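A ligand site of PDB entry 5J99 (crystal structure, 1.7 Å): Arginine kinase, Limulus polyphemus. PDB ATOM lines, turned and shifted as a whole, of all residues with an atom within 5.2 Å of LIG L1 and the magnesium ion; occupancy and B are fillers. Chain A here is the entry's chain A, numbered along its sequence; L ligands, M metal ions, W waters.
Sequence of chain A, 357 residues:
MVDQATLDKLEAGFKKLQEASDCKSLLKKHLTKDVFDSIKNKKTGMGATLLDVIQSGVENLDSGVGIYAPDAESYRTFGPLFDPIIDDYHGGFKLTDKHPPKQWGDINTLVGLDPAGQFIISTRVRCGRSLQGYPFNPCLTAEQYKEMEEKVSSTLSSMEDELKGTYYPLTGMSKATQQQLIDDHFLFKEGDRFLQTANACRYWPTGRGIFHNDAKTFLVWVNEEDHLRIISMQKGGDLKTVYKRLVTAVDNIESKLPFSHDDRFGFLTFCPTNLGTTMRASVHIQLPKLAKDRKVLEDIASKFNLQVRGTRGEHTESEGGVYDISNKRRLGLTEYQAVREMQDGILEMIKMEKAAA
Water W8 lies within hydrogen-bond range of the side-chain carboxylate (OE1) of Glu 224 (2.8 Å), the side-chain carboxylate (OE2) of Glu 225 (2.9 Å) and the guanidinium group (NH1) of Arg 229 (3.3 Å). Water W6 lies within hydrogen-bond range of O2 of LIG L1 (2.6 Å) and NH1 of Arg 229 (2.9 Å). Water W1 lies within hydrogen-bond range of O9 of LIG L1, O of Ile 182 and ND1 of His 185. Water W4 lies within hydrogen-bond range of the backbone carbonyl oxygen (O) of Leu 187 (2.8 Å) and an oxygen (O9) of LIG L1 (2.8 Å). Water W3 lies within hydrogen-bond range of OD2 of Asp 324, NE2 of His 284, O of Thr 311, O10 of LIG L1 and N of Gly 313.
The backbone NH (N) of His 284 lies close to a nitrogen (N3) of LIG L1, at 3.3 Å. The side-chain carboxylate (OD2) of Asp 324 lies close to a nitrogen (N2) of LIG L1, at 3.5 Å. CH2 of Trp 221 touches C1 of LIG L1, 3.7 Å away. Met 233 touches LIG L1 (CE to C9, 3.8 Å). Val 283 touches LIG L1 (C to N3, 3.4 Å). C of Arg 312 touches O10 of LIG L1, 3.7 Å away. Gly 313 touches LIG L1 (CA to O4, 3.3 Å).
No residue comes within 4 Å of the magnesium ion. The nearest printed residue that does not touch the magnesium ion is Glu 224 (4.1 Å).
The backbone carbonyl oxygen of Ser 122 sits at hydrogen-bond distance from the backbone NH of His 284. The backbone carbonyl oxygen (O) of Arg 124 sits at hydrogen-bond distance from the backbone NH (N) of Ser 282, 2.8 Å away. O of Thr 311 lies close to NE2 of His 284 (3.4 Å). N of Arg 309 sits at hydrogen-bond distance from O of Asp 324 (2.7 Å). The backbone carbonyl oxygen of Arg 229 is in hydrogen-bond range of the backbone NH of Trp 221 (2.9 Å). NH2 of Arg 229 lies within salt-bridge range of OE1 of Glu 225. The guanidinium group (NH1) of Arg 280 is in salt-bridge range of the side-chain carboxylate (OD1) of Asp 324 (2.9 Å). The indole nitrogen (NE1) of Trp 221 sits at hydrogen-bond distance from the backbone carbonyl oxygen (O) of Phe 186 (2.8 Å).
The magnesium ion is bound by O3 of LIG L1 (2.0 Å), water W2 (2.1 Å), O5 of LIG L1 (2.1 Å), water W8 (2.1 Å), water W5 (2.1 Å) and O1 of LG2 L2 (2.5 Å).
The guanidinium group of Arg 126 is in salt-bridge range of an oxygen (O1) of LIG L1 (2.6 Å). A nitrogen (N3) of LIG L1 sits at hydrogen-bond distance from the backbone carbonyl oxygen (O) of Ser 122, at 3.2 Å. The side-chain hydroxyl (OG) of Ser 122 sits at hydrogen-bond distance from a nitrogen (N4) of LIG L1 (2.7 Å). N3 of LIG L1 lies within hydrogen-bond range of O of Ser 282 (3.3 Å). OG of Ser 282 sits at hydrogen-bond distance from N2 of LIG L1, at 2.7 Å. An oxygen (O2) of LIG L1 is in salt-bridge range of the guanidinium group of Arg 124, 2.8 Å away. O of Thr 311 lies within hydrogen-bond range of O10 of LIG L1, 2.8 Å away. An oxygen (O4) of LIG L1 lies within salt-bridge range of the guanidinium group of Arg 309, 2.8 Å away. N of Glu 314 lies within hydrogen-bond range of O4 of LIG L1 (2.9 Å). ND1 of His 185 lies within hydrogen-bond range of O10 of LIG L1, at 3.0 Å. NH1 of Arg 229 is in salt-bridge range of O1 of LIG L1, 3.8 Å away. The guanidinium group of Arg 280 is in salt-bridge range of an oxygen (O1) of LIG L1 (3.0 Å). OE1 of Glu 314 lies within salt-bridge range of N2 of LG3 L3 (3.0 Å). N3 of LG3 L3 lies within salt-bridge range of OE2 of Glu 225 (2.7 Å).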
ATOM      1  N   SER A 122      10.541 -34.531  -5.875  1.00  0.00           N
ATOM      2  CA  SER A 122      11.045 -35.023  -4.586  1.00  0.00           C
ATOM      3  C   SER A 122       9.911 -35.098  -3.541  1.00  0.00           C
ATOM      4  O   SER A 122       8.911 -34.352  -3.612  1.00  0.00           O
ATOM      5  CB  SER A 122      12.184 -34.124  -4.072  1.00  0.00           C
ATOM      6  OG  SER A 122      11.721 -32.783  -3.924  1.00  0.00           O
ATOM      7  N   THR A 123      10.074 -36.012  -2.588  1.00  0.00           N
ATOM      8  CA  THR A 123       9.043 -36.300  -1.597  1.00  0.00           C
ATOM      9  C   THR A 123       9.645 -36.135  -0.211  1.00  0.00           C
ATOM     10  O   THR A 123      10.768 -36.550   0.038  1.00  0.00           O
ATOM     11  CB  THR A 123       8.502 -37.723  -1.746  1.00  0.00           C
ATOM     12  OG1 THR A 123       7.963 -37.881  -3.069  1.00  0.00           O
ATOM     13  CG2 THR A 123       7.397 -37.968  -0.695  1.00  0.00           C
ATOM     14  N   ARG A 124       8.911 -35.542   0.705  1.00  0.00           N
ATOM     15  CA  ARG A 124       9.496 -35.203   2.014  1.00  0.00           C
ATOM     16  C   ARG A 124       8.412 -35.414   3.058  1.00  0.00           C
ATOM     17  O   ARG A 124       7.277 -35.028   2.854  1.00  0.00           O
ATOM     18  CB  ARG A 124       9.933 -33.753   2.052  1.00  0.00           C
ATOM     19  CG  ARG A 124      10.432 -33.263   3.440  1.00  0.00           C
ATOM     20  CD  ARG A 124      10.930 -31.846   3.160  1.00  0.00           C
ATOM     21  NE  ARG A 124      11.578 -31.109   4.259  1.00  0.00           N
ATOM     22  CZ  ARG A 124      10.952 -30.323   5.129  1.00  0.00           C
ATOM     23  NH1 ARG A 124       9.616 -30.194   5.110  1.00  0.00           N
ATOM     24  NH2 ARG A 124      11.695 -29.624   6.036  1.00  0.00           N
ATOM     25  N   ARG A 126       7.865 -34.697   7.247  1.00  0.00           N
ATOM     26  CA  ARG A 126       8.474 -34.259   8.530  1.00  0.00           C
ATOM     27  C   ARG A 126       7.501 -34.315   9.692  1.00  0.00           C
ATOM     28  O   ARG A 126       6.287 -34.214   9.492  1.00  0.00           O
ATOM     29  CB  ARG A 126       9.089 -32.851   8.380  1.00  0.00           C
ATOM     30  CG  ARG A 126       8.091 -31.692   8.094  1.00  0.00           C
ATOM     31  CD  ARG A 126       7.395 -31.148   9.395  1.00  0.00           C
ATOM     32  NE  ARG A 126       6.805 -29.822   9.117  1.00  0.00           N
ATOM     33  CZ  ARG A 126       5.744 -29.295   9.718  1.00  0.00           C
ATOM     34  NH1 ARG A 126       5.344 -28.051   9.386  1.00  0.00           N
ATOM     35  NH2 ARG A 126       5.091 -29.980  10.650  1.00  0.00           N
ATOM     36  N   ILE A 182      20.821 -24.716   2.424  1.00  0.00           N
ATOM     37  CA  ILE A 182      19.515 -24.079   2.313  1.00  0.00           C
ATOM     38  C   ILE A 182      19.022 -24.150   0.862  1.00  0.00           C
ATOM     39  O   ILE A 182      17.863 -24.513   0.607  1.00  0.00           O
ATOM     40  CB  ILE A 182      19.545 -22.586   2.800  1.00  0.00           C
ATOM     41  CG1 ILE A 182      19.744 -22.519   4.320  1.00  0.00           C
ATOM     42  CG2 ILE A 182      18.181 -21.925   2.506  1.00  0.00           C
ATOM     43  CD1 ILE A 182      20.020 -21.120   4.810  1.00  0.00           C
ATOM     44  N   HIS A 185      17.572 -27.372  -0.124  1.00  0.00           N
ATOM     45  CA  HIS A 185      16.314 -27.717   0.564  1.00  0.00           C
ATOM     46  C   HIS A 185      16.472 -28.549   1.819  1.00  0.00           C
ATOM     47  O   HIS A 185      15.508 -29.116   2.317  1.00  0.00           O
ATOM     48  CB  HIS A 185      15.342 -28.446  -0.377  1.00  0.00           C
ATOM     49  CG  HIS A 185      15.107 -27.720  -1.666  1.00  0.00           C
ATOM     50  ND1 HIS A 185      14.483 -26.496  -1.718  1.00  0.00           N
ATOM     51  CD2 HIS A 185      15.454 -28.022  -2.939  1.00  0.00           C
ATOM     52  CE1 HIS A 185      14.445 -26.069  -2.975  1.00  0.00           C
ATOM     53  NE2 HIS A 185      15.023 -26.980  -3.736  1.00  0.00           N
ATOM     54  N   PHE A 186      17.683 -28.624   2.353  1.00  0.00           N
ATOM     55  CA  PHE A 186      17.971 -29.463   3.497  1.00  0.00           C
ATOM     56  C   PHE A 186      17.849 -28.703   4.803  1.00  0.00           C
ATOM     57  O   PHE A 186      17.271 -29.201   5.762  1.00  0.00           O
ATOM     58  CB  PHE A 186      19.382 -30.048   3.363  1.00  0.00           C
ATOM     59  CG  PHE A 186      19.530 -30.994   2.209  1.00  0.00           C
ATOM     60  CD1 PHE A 186      18.574 -31.989   1.966  1.00  0.00           C
ATOM     61  CD2 PHE A 186      20.571 -30.842   1.311  1.00  0.00           C
ATOM     62  CE1 PHE A 186      18.729 -32.852   0.873  1.00  0.00           C
ATOM     63  CE2 PHE A 186      20.714 -31.686   0.219  1.00  0.00           C
ATOM     64  CZ  PHE A 186      19.795 -32.690  -0.005  1.00  0.00           C
ATOM     65  N   LEU A 187      18.426 -27.504   4.844  1.00  0.00           N
ATOM     66  CA  LEU A 187      18.538 -26.735   6.074  1.00  0.00           C
ATOM     67  C   LEU A 187      17.519 -25.604   6.127  1.00  0.00           C
ATOM     68  O   LEU A 187      17.171 -25.034   5.092  1.00  0.00           O
ATOM     69  CB  LEU A 187      19.987 -26.171   6.169  1.00  0.00           C
ATOM     70  CG  LEU A 187      20.336 -25.256   7.351  1.00  0.00           C
ATOM     71  CD1 LEU A 187      20.267 -25.991   8.673  1.00  0.00           C
ATOM     72  CD2 LEU A 187      21.743 -24.688   7.146  1.00  0.00           C
ATOM     73  N   TRP A 221      16.402 -31.215  12.386  1.00  0.00           N
ATOM     74  CA  TRP A 221      16.686 -29.811  12.719  1.00  0.00           C
ATOM     75  C   TRP A 221      16.566 -29.608  14.191  1.00  0.00           C
ATOM     76  O   TRP A 221      15.567 -30.003  14.799  1.00  0.00           O
ATOM     77  CB  TRP A 221      15.699 -28.850  12.036  1.00  0.00           C
ATOM     78  CG  TRP A 221      15.674 -28.812  10.546  1.00  0.00           C
ATOM     79  CD1 TRP A 221      16.611 -29.307   9.669  1.00  0.00           C
ATOM     80  CD2 TRP A 221      14.715 -28.105   9.757  1.00  0.00           C
ATOM     81  NE1 TRP A 221      16.261 -28.971   8.384  1.00  0.00           N
ATOM     82  CE2 TRP A 221      15.107 -28.226   8.405  1.00  0.00           C
ATOM     83  CE3 TRP A 221      13.572 -27.368  10.077  1.00  0.00           C
ATOM     84  CZ2 TRP A 221      14.366 -27.667   7.354  1.00  0.00           C
ATOM     85  CZ3 TRP A 221      12.832 -26.797   9.019  1.00  0.00           C
ATOM     86  CH2 TRP A 221      13.220 -26.963   7.689  1.00  0.00           C
ATOM     87  N   GLU A 224      15.017 -24.845  15.667  1.00  0.00           N
ATOM     88  CA  GLU A 224      14.453 -23.816  14.796  1.00  0.00           C
ATOM     89  C   GLU A 224      13.057 -23.484  15.363  1.00  0.00           C
ATOM     90  O   GLU A 224      12.937 -23.009  16.484  1.00  0.00           O
ATOM     91  CB  GLU A 224      14.403 -24.286  13.346  1.00  0.00           C
ATOM     92  CG  GLU A 224      14.102 -23.173  12.327  1.00  0.00           C
ATOM     93  CD  GLU A 224      12.880 -23.489  11.435  1.00  0.00           C
ATOM     94  OE1 GLU A 224      12.046 -24.373  11.782  1.00  0.00           O
ATOM     95  OE2 GLU A 224      12.770 -22.856  10.368  1.00  0.00           O
ATOM     96  N   GLU A 225      11.996 -23.807  14.625  1.00  0.00           N
ATOM     97  CA  GLU A 225      10.664 -23.408  15.076  1.00  0.00           C
ATOM     98  C   GLU A 225      10.236 -24.274  16.263  1.00  0.00           C
ATOM     99  O   GLU A 225       9.718 -23.754  17.273  1.00  0.00           O
ATOM    100  CB  GLU A 225       9.676 -23.519  13.902  1.00  0.00           C
ATOM    101  CG  GLU A 225       8.233 -23.231  14.393  1.00  0.00           C
ATOM    102  CD  GLU A 225       7.260 -23.254  13.252  1.00  0.00           C
ATOM    103  OE1 GLU A 225       6.081 -23.551  13.516  1.00  0.00           O
ATOM    104  OE2 GLU A 225       7.678 -22.957  12.108  1.00  0.00           O
ATOM    105  N   ARG A 229      12.728 -30.975  14.561  1.00  0.00           N
ATOM    106  CA  ARG A 229      11.970 -31.406  13.384  1.00  0.00           C
ATOM    107  C   ARG A 229      12.687 -32.622  12.839  1.00  0.00           C
ATOM    108  O   ARG A 229      13.899 -32.600  12.658  1.00  0.00           O
ATOM    109  CB  ARG A 229      11.915 -30.330  12.325  1.00  0.00           C
ATOM    110  CG  ARG A 229      11.097 -29.142  12.728  1.00  0.00           C
ATOM    111  CD  ARG A 229       9.597 -29.476  12.684  1.00  0.00           C
ATOM    112  NE  ARG A 229       8.804 -28.287  13.041  1.00  0.00           N
ATOM    113  CZ  ARG A 229       8.460 -27.344  12.156  1.00  0.00           C
ATOM    114  NH1 ARG A 229       8.876 -27.436  10.891  1.00  0.00           N
ATOM    115  NH2 ARG A 229       7.699 -26.320  12.543  1.00  0.00           N
ATOM    116  N   MET A 233      13.450 -37.476   3.393  1.00  0.00           N
ATOM    117  CA  MET A 233      13.205 -36.913   2.036  1.00  0.00           C
ATOM    118  C   MET A 233      14.121 -37.555   0.985  1.00  0.00           C
ATOM    119  O   MET A 233      15.208 -38.062   1.332  1.00  0.00           O
ATOM    120  CB  MET A 233      13.387 -35.383   2.034  1.00  0.00           C
ATOM    121  CG  MET A 233      14.778 -34.921   2.400  1.00  0.00           C
ATOM    122  SD  MET A 233      14.743 -33.108   2.632  1.00  0.00           S
ATOM    123  CE  MET A 233      14.944 -32.502   0.952  1.00  0.00           C
ATOM    124  N   ARG A 280       3.826 -33.050   8.251  1.00  0.00           N
ATOM    125  CA  ARG A 280       3.639 -32.379   6.955  1.00  0.00           C
ATOM    126  C   ARG A 280       4.321 -33.259   5.892  1.00  0.00           C
ATOM    127  O   ARG A 280       5.553 -33.421   5.915  1.00  0.00           O
ATOM    128  CB  ARG A 280       4.208 -30.978   6.949  1.00  0.00           C
ATOM    129  CG  ARG A 280       3.827 -30.221   5.685  1.00  0.00           C
ATOM    130  CD  ARG A 280       4.156 -28.713   5.788  1.00  0.00           C
ATOM    131  NE  ARG A 280       5.495 -28.393   5.247  1.00  0.00           N
ATOM    132  CZ  ARG A 280       5.739 -28.212   3.942  1.00  0.00           C
ATOM    133  NH1 ARG A 280       4.785 -28.425   3.046  1.00  0.00           N
ATOM    134  NH2 ARG A 280       6.937 -27.853   3.506  1.00  0.00           N
ATOM    135  N   SER A 282       4.956 -33.715   1.973  1.00  0.00           N
ATOM    136  CA  SER A 282       4.904 -32.846   0.810  1.00  0.00           C
ATOM    137  C   SER A 282       5.588 -33.446  -0.410  1.00  0.00           C
ATOM    138  O   SER A 282       6.420 -34.347  -0.315  1.00  0.00           O
ATOM    139  CB  SER A 282       5.537 -31.499   1.111  1.00  0.00           C
ATOM    140  OG  SER A 282       6.953 -31.671   1.316  1.00  0.00           O
ATOM    141  N   VAL A 283       5.205 -32.948  -1.587  1.00  0.00           N
ATOM    142  CA  VAL A 283       5.945 -33.203  -2.817  1.00  0.00           C
ATOM    143  C   VAL A 283       6.335 -31.880  -3.404  1.00  0.00           C
ATOM    144  O   VAL A 283       5.646 -30.867  -3.210  1.00  0.00           O
ATOM    145  CB  VAL A 283       5.135 -33.994  -3.827  1.00  0.00           C
ATOM    146  CG1 VAL A 283       4.928 -35.424  -3.333  1.00  0.00           C
ATOM    147  CG2 VAL A 283       3.751 -33.356  -4.057  1.00  0.00           C
ATOM    148  N   HIS A 284       7.470 -31.857  -4.075  1.00  0.00           N
ATOM    149  CA  HIS A 284       7.789 -30.788  -5.021  1.00  0.00           C
ATOM    150  C   HIS A 284       7.318 -31.324  -6.356  1.00  0.00           C
ATOM    151  O   HIS A 284       7.706 -32.425  -6.776  1.00  0.00           O
ATOM    152  CB  HIS A 284       9.286 -30.492  -5.061  1.00  0.00           C
ATOM    153  CG  HIS A 284       9.693 -29.461  -4.051  1.00  0.00           C
ATOM    154  ND1 HIS A 284      10.947 -28.873  -4.042  1.00  0.00           N
ATOM    155  CD2 HIS A 284       9.013 -28.910  -3.031  1.00  0.00           C
ATOM    156  CE1 HIS A 284      11.002 -27.990  -3.052  1.00  0.00           C
ATOM    157  NE2 HIS A 284       9.846 -28.000  -2.416  1.00  0.00           N
ATOM    158  N   ARG A 309       2.684 -24.228  -1.206  1.00  0.00           N
ATOM    159  CA  ARG A 309       3.797 -23.333  -0.807  1.00  0.00           C
ATOM    160  C   ARG A 309       4.773 -23.166  -1.966  1.00  0.00           C
ATOM    161  O   ARG A 309       4.758 -23.972  -2.897  1.00  0.00           O
ATOM    162  CB  ARG A 309       4.542 -23.939   0.406  1.00  0.00           C
ATOM    163  CG  ARG A 309       3.748 -23.991   1.665  1.00  0.00           C
ATOM    164  CD  ARG A 309       4.557 -24.688   2.794  1.00  0.00           C
ATOM    165  NE  ARG A 309       3.685 -24.844   3.955  1.00  0.00           N
ATOM    166  CZ  ARG A 309       4.095 -24.985   5.212  1.00  0.00           C
ATOM    167  NH1 ARG A 309       5.406 -24.954   5.478  1.00  0.00           N
ATOM    168  NH2 ARG A 309       3.199 -25.090   6.174  1.00  0.00           N
ATOM    169  N   THR A 311       8.728 -22.817  -3.812  1.00  0.00           N
ATOM    170  CA  THR A 311       9.773 -23.822  -3.938  1.00  0.00           C
ATOM    171  C   THR A 311      10.745 -23.821  -2.728  1.00  0.00           C
ATOM    172  O   THR A 311      11.293 -24.875  -2.334  1.00  0.00           O
ATOM    173  CB  THR A 311      10.558 -23.591  -5.239  1.00  0.00           C
ATOM    174  OG1 THR A 311       9.635 -23.364  -6.315  1.00  0.00           O
ATOM    175  CG2 THR A 311      11.442 -24.787  -5.548  1.00  0.00           C
ATOM    176  N   ARG A 312      10.946 -22.665  -2.118  1.00  0.00           N
ATOM    177  CA  ARG A 312      11.860 -22.579  -0.971  1.00  0.00           C
ATOM    178  C   ARG A 312      11.112 -22.581   0.333  1.00  0.00           C
ATOM    179  O   ARG A 312      11.667 -22.200   1.364  1.00  0.00           O
ATOM    180  CB  ARG A 312      12.736 -21.309  -1.091  1.00  0.00           C
ATOM    181  CG  ARG A 312      13.575 -21.350  -2.376  1.00  0.00           C
ATOM    182  CD  ARG A 312      14.365 -20.059  -2.561  1.00  0.00           C
ATOM    183  NE  ARG A 312      15.586 -20.074  -1.767  1.00  0.00           N
ATOM    184  CZ  ARG A 312      16.717 -20.681  -2.140  1.00  0.00           C
ATOM    185  NH1 ARG A 312      16.774 -21.341  -3.296  1.00  0.00           N
ATOM    186  NH2 ARG A 312      17.775 -20.643  -1.342  1.00  0.00           N
ATOM    187  N   GLY A 313       9.847 -22.991   0.292  1.00  0.00           N
ATOM    188  CA  GLY A 313       9.090 -23.146   1.521  1.00  0.00           C
ATOM    189  C   GLY A 313       7.966 -22.121   1.659  1.00  0.00           C
ATOM    190  O   GLY A 313       7.654 -21.378   0.712  1.00  0.00           O
ATOM    191  N   GLU A 314       7.325 -22.099   2.820  1.00  0.00           N
ATOM    192  CA  GLU A 314       6.206 -21.145   2.957  1.00  0.00           C
ATOM    193  C   GLU A 314       6.682 -19.695   2.772  1.00  0.00           C
ATOM    194  O   GLU A 314       7.858 -19.374   3.045  1.00  0.00           O
ATOM    195  CB  GLU A 314       5.542 -21.291   4.322  1.00  0.00           C
ATOM    196  CG  GLU A 314       6.580 -21.228   5.447  1.00  0.00           C
ATOM    197  CD  GLU A 314       5.898 -21.165   6.828  1.00  0.00           C
ATOM    198  OE1 GLU A 314       4.628 -21.211   6.868  1.00  0.00           O
ATOM    199  OE2 GLU A 314       6.637 -21.085   7.834  1.00  0.00           O
ATOM    200  N   ASP A 324       5.345 -26.745  -3.801  1.00  0.00           N
ATOM    201  CA  ASP A 324       5.300 -27.595  -2.633  1.00  0.00           C
ATOM    202  C   ASP A 324       3.846 -27.785  -2.283  1.00  0.00           C
ATOM    203  O   ASP A 324       3.157 -26.816  -1.948  1.00  0.00           O
ATOM    204  CB  ASP A 324       6.117 -26.880  -1.530  1.00  0.00           C
ATOM    205  CG  ASP A 324       6.000 -27.499  -0.145  1.00  0.00           C
ATOM    206  OD1 ASP A 324       5.067 -28.239   0.190  1.00  0.00           O
ATOM    207  OD2 ASP A 324       6.900 -27.154   0.665  1.00  0.00           O
HETATM  208  P1  LIG L   1       8.530 -27.111   7.201  1.00  0.00           P
HETATM  209  O1  LIG L   1       7.102 -27.332   7.574  1.00  0.00           O
HETATM  210  O2  LIG L   1       9.361 -28.379   7.170  1.00  0.00           O
HETATM  211  O3  LIG L   1       9.256 -26.194   8.189  1.00  0.00           O
HETATM  212  P2  LIG L   1       8.971 -25.046   5.118  1.00  0.00           P
HETATM  213  O4  LIG L   1       7.879 -24.557   4.192  1.00  0.00           O
HETATM  214  O5  LIG L   1       9.469 -24.129   6.260  1.00  0.00           O
HETATM  215  O6  LIG L   1       8.526 -26.472   5.731  1.00  0.00           O
HETATM  216  O7  LIG L   1      10.130 -25.466   4.121  1.00  0.00           O
HETATM  217  C1  LIG L   1      11.318 -26.060   4.694  1.00  0.00           C
HETATM  218  C2  LIG L   1      12.248 -26.573   3.609  1.00  0.00           C
HETATM  219  O8  LIG L   1      11.755 -27.831   3.113  1.00  0.00           O
HETATM  220  C3  LIG L   1      12.399 -25.647   2.423  1.00  0.00           C
HETATM  221  O9  LIG L   1      13.762 -25.586   1.988  1.00  0.00           O
HETATM  222  C4  LIG L   1      11.601 -26.351   1.328  1.00  0.00           C
HETATM  223  O10 LIG L   1      12.136 -26.101   0.051  1.00  0.00           O
HETATM  224  C5  LIG L   1      11.822 -27.784   1.696  1.00  0.00           C
HETATM  225  N1  LIG L   1      10.834 -28.748   1.182  1.00  0.00           N
HETATM  226  C6  LIG L   1       9.540 -28.865   1.574  1.00  0.00           C
HETATM  227  N2  LIG L   1       8.988 -29.927   0.898  1.00  0.00           N
HETATM  228  C7  LIG L   1       9.939 -30.429   0.076  1.00  0.00           C
HETATM  229  C8  LIG L   1      10.001 -31.524  -0.910  1.00  0.00           C
HETATM  230  N3  LIG L   1       8.917 -32.298  -1.159  1.00  0.00           N
HETATM  231  N4  LIG L   1      11.181 -31.721  -1.516  1.00  0.00           N
HETATM  232  C9  LIG L   1      12.283 -30.977  -1.320  1.00  0.00           C
HETATM  233  N5  LIG L   1      12.280 -29.971  -0.440  1.00  0.00           N
HETATM  234  C10 LIG L   1      11.148 -29.651   0.258  1.00  0.00           C
HETATM  235  N1  LG2 L   2       6.081 -24.943   9.090  1.00  0.00           N
HETATM  236  O1  LG2 L   2       6.937 -24.340   8.363  1.00  0.00           O
HETATM  237  O2  LG2 L   2       4.869 -25.096   8.702  1.00  0.00           O
HETATM  238  O3  LG2 L   2       6.439 -25.388  10.238  1.00  0.00           O
HETATM  239  N1  LG3 L   3       3.192 -17.046  11.558  1.00  0.00           N
HETATM  240  C1  LG3 L   3       3.113 -17.341  10.134  1.00  0.00           C
HETATM  241  C2  LG3 L   3       1.737 -16.968   9.599  1.00  0.00           C
HETATM  242  O1  LG3 L   3       0.849 -16.583  10.374  1.00  0.00           O
HETATM  243  C3  LG3 L   3       3.412 -18.823   9.867  1.00  0.00           C
HETATM  244  C4  LG3 L   3       2.371 -19.769  10.448  1.00  0.00           C
HETATM  245  C5  LG3 L   3       2.350 -21.108   9.771  1.00  0.00           C
HETATM  246  N2  LG3 L   3       3.703 -21.629   9.643  1.00  0.00           N
HETATM  247  C6  LG3 L   3       4.407 -22.174  10.642  1.00  0.00           C
HETATM  248  N3  LG3 L   3       5.650 -22.578  10.408  1.00  0.00           N
HETATM  249  N4  LG3 L   3       3.905 -22.250  11.879  1.00  0.00           N
HETATM  250  O2  LG3 L   3       1.523 -17.037   8.392  1.00  0.00           O
HETATM  251 MG    MG M   1       9.434 -24.190   8.344  1.00  0.00          MG
HETATM  252  O   HOH W   1      15.004 -23.961   0.146  1.00  0.00           O
HETATM  253  O   HOH W   2      11.494 -23.894   8.252  1.00  0.00           O
HETATM  254  O   HOH W   3       9.054 -26.068  -0.507  1.00  0.00           O
HETATM  255  O   HOH W   4      14.886 -23.921   3.969  1.00  0.00           O
HETATM  256  O   HOH W   5       9.151 -22.074   8.242  1.00  0.00           O
HETATM  257  O   HOH W   6      10.498 -29.213   9.350  1.00  0.00           O
HETATM  258  O   HOH W   7      10.802 -21.691   5.735  1.00  0.00           O
HETATM  259  O   HOH W   8       9.643 -24.297  10.429  1.00  0.00           O
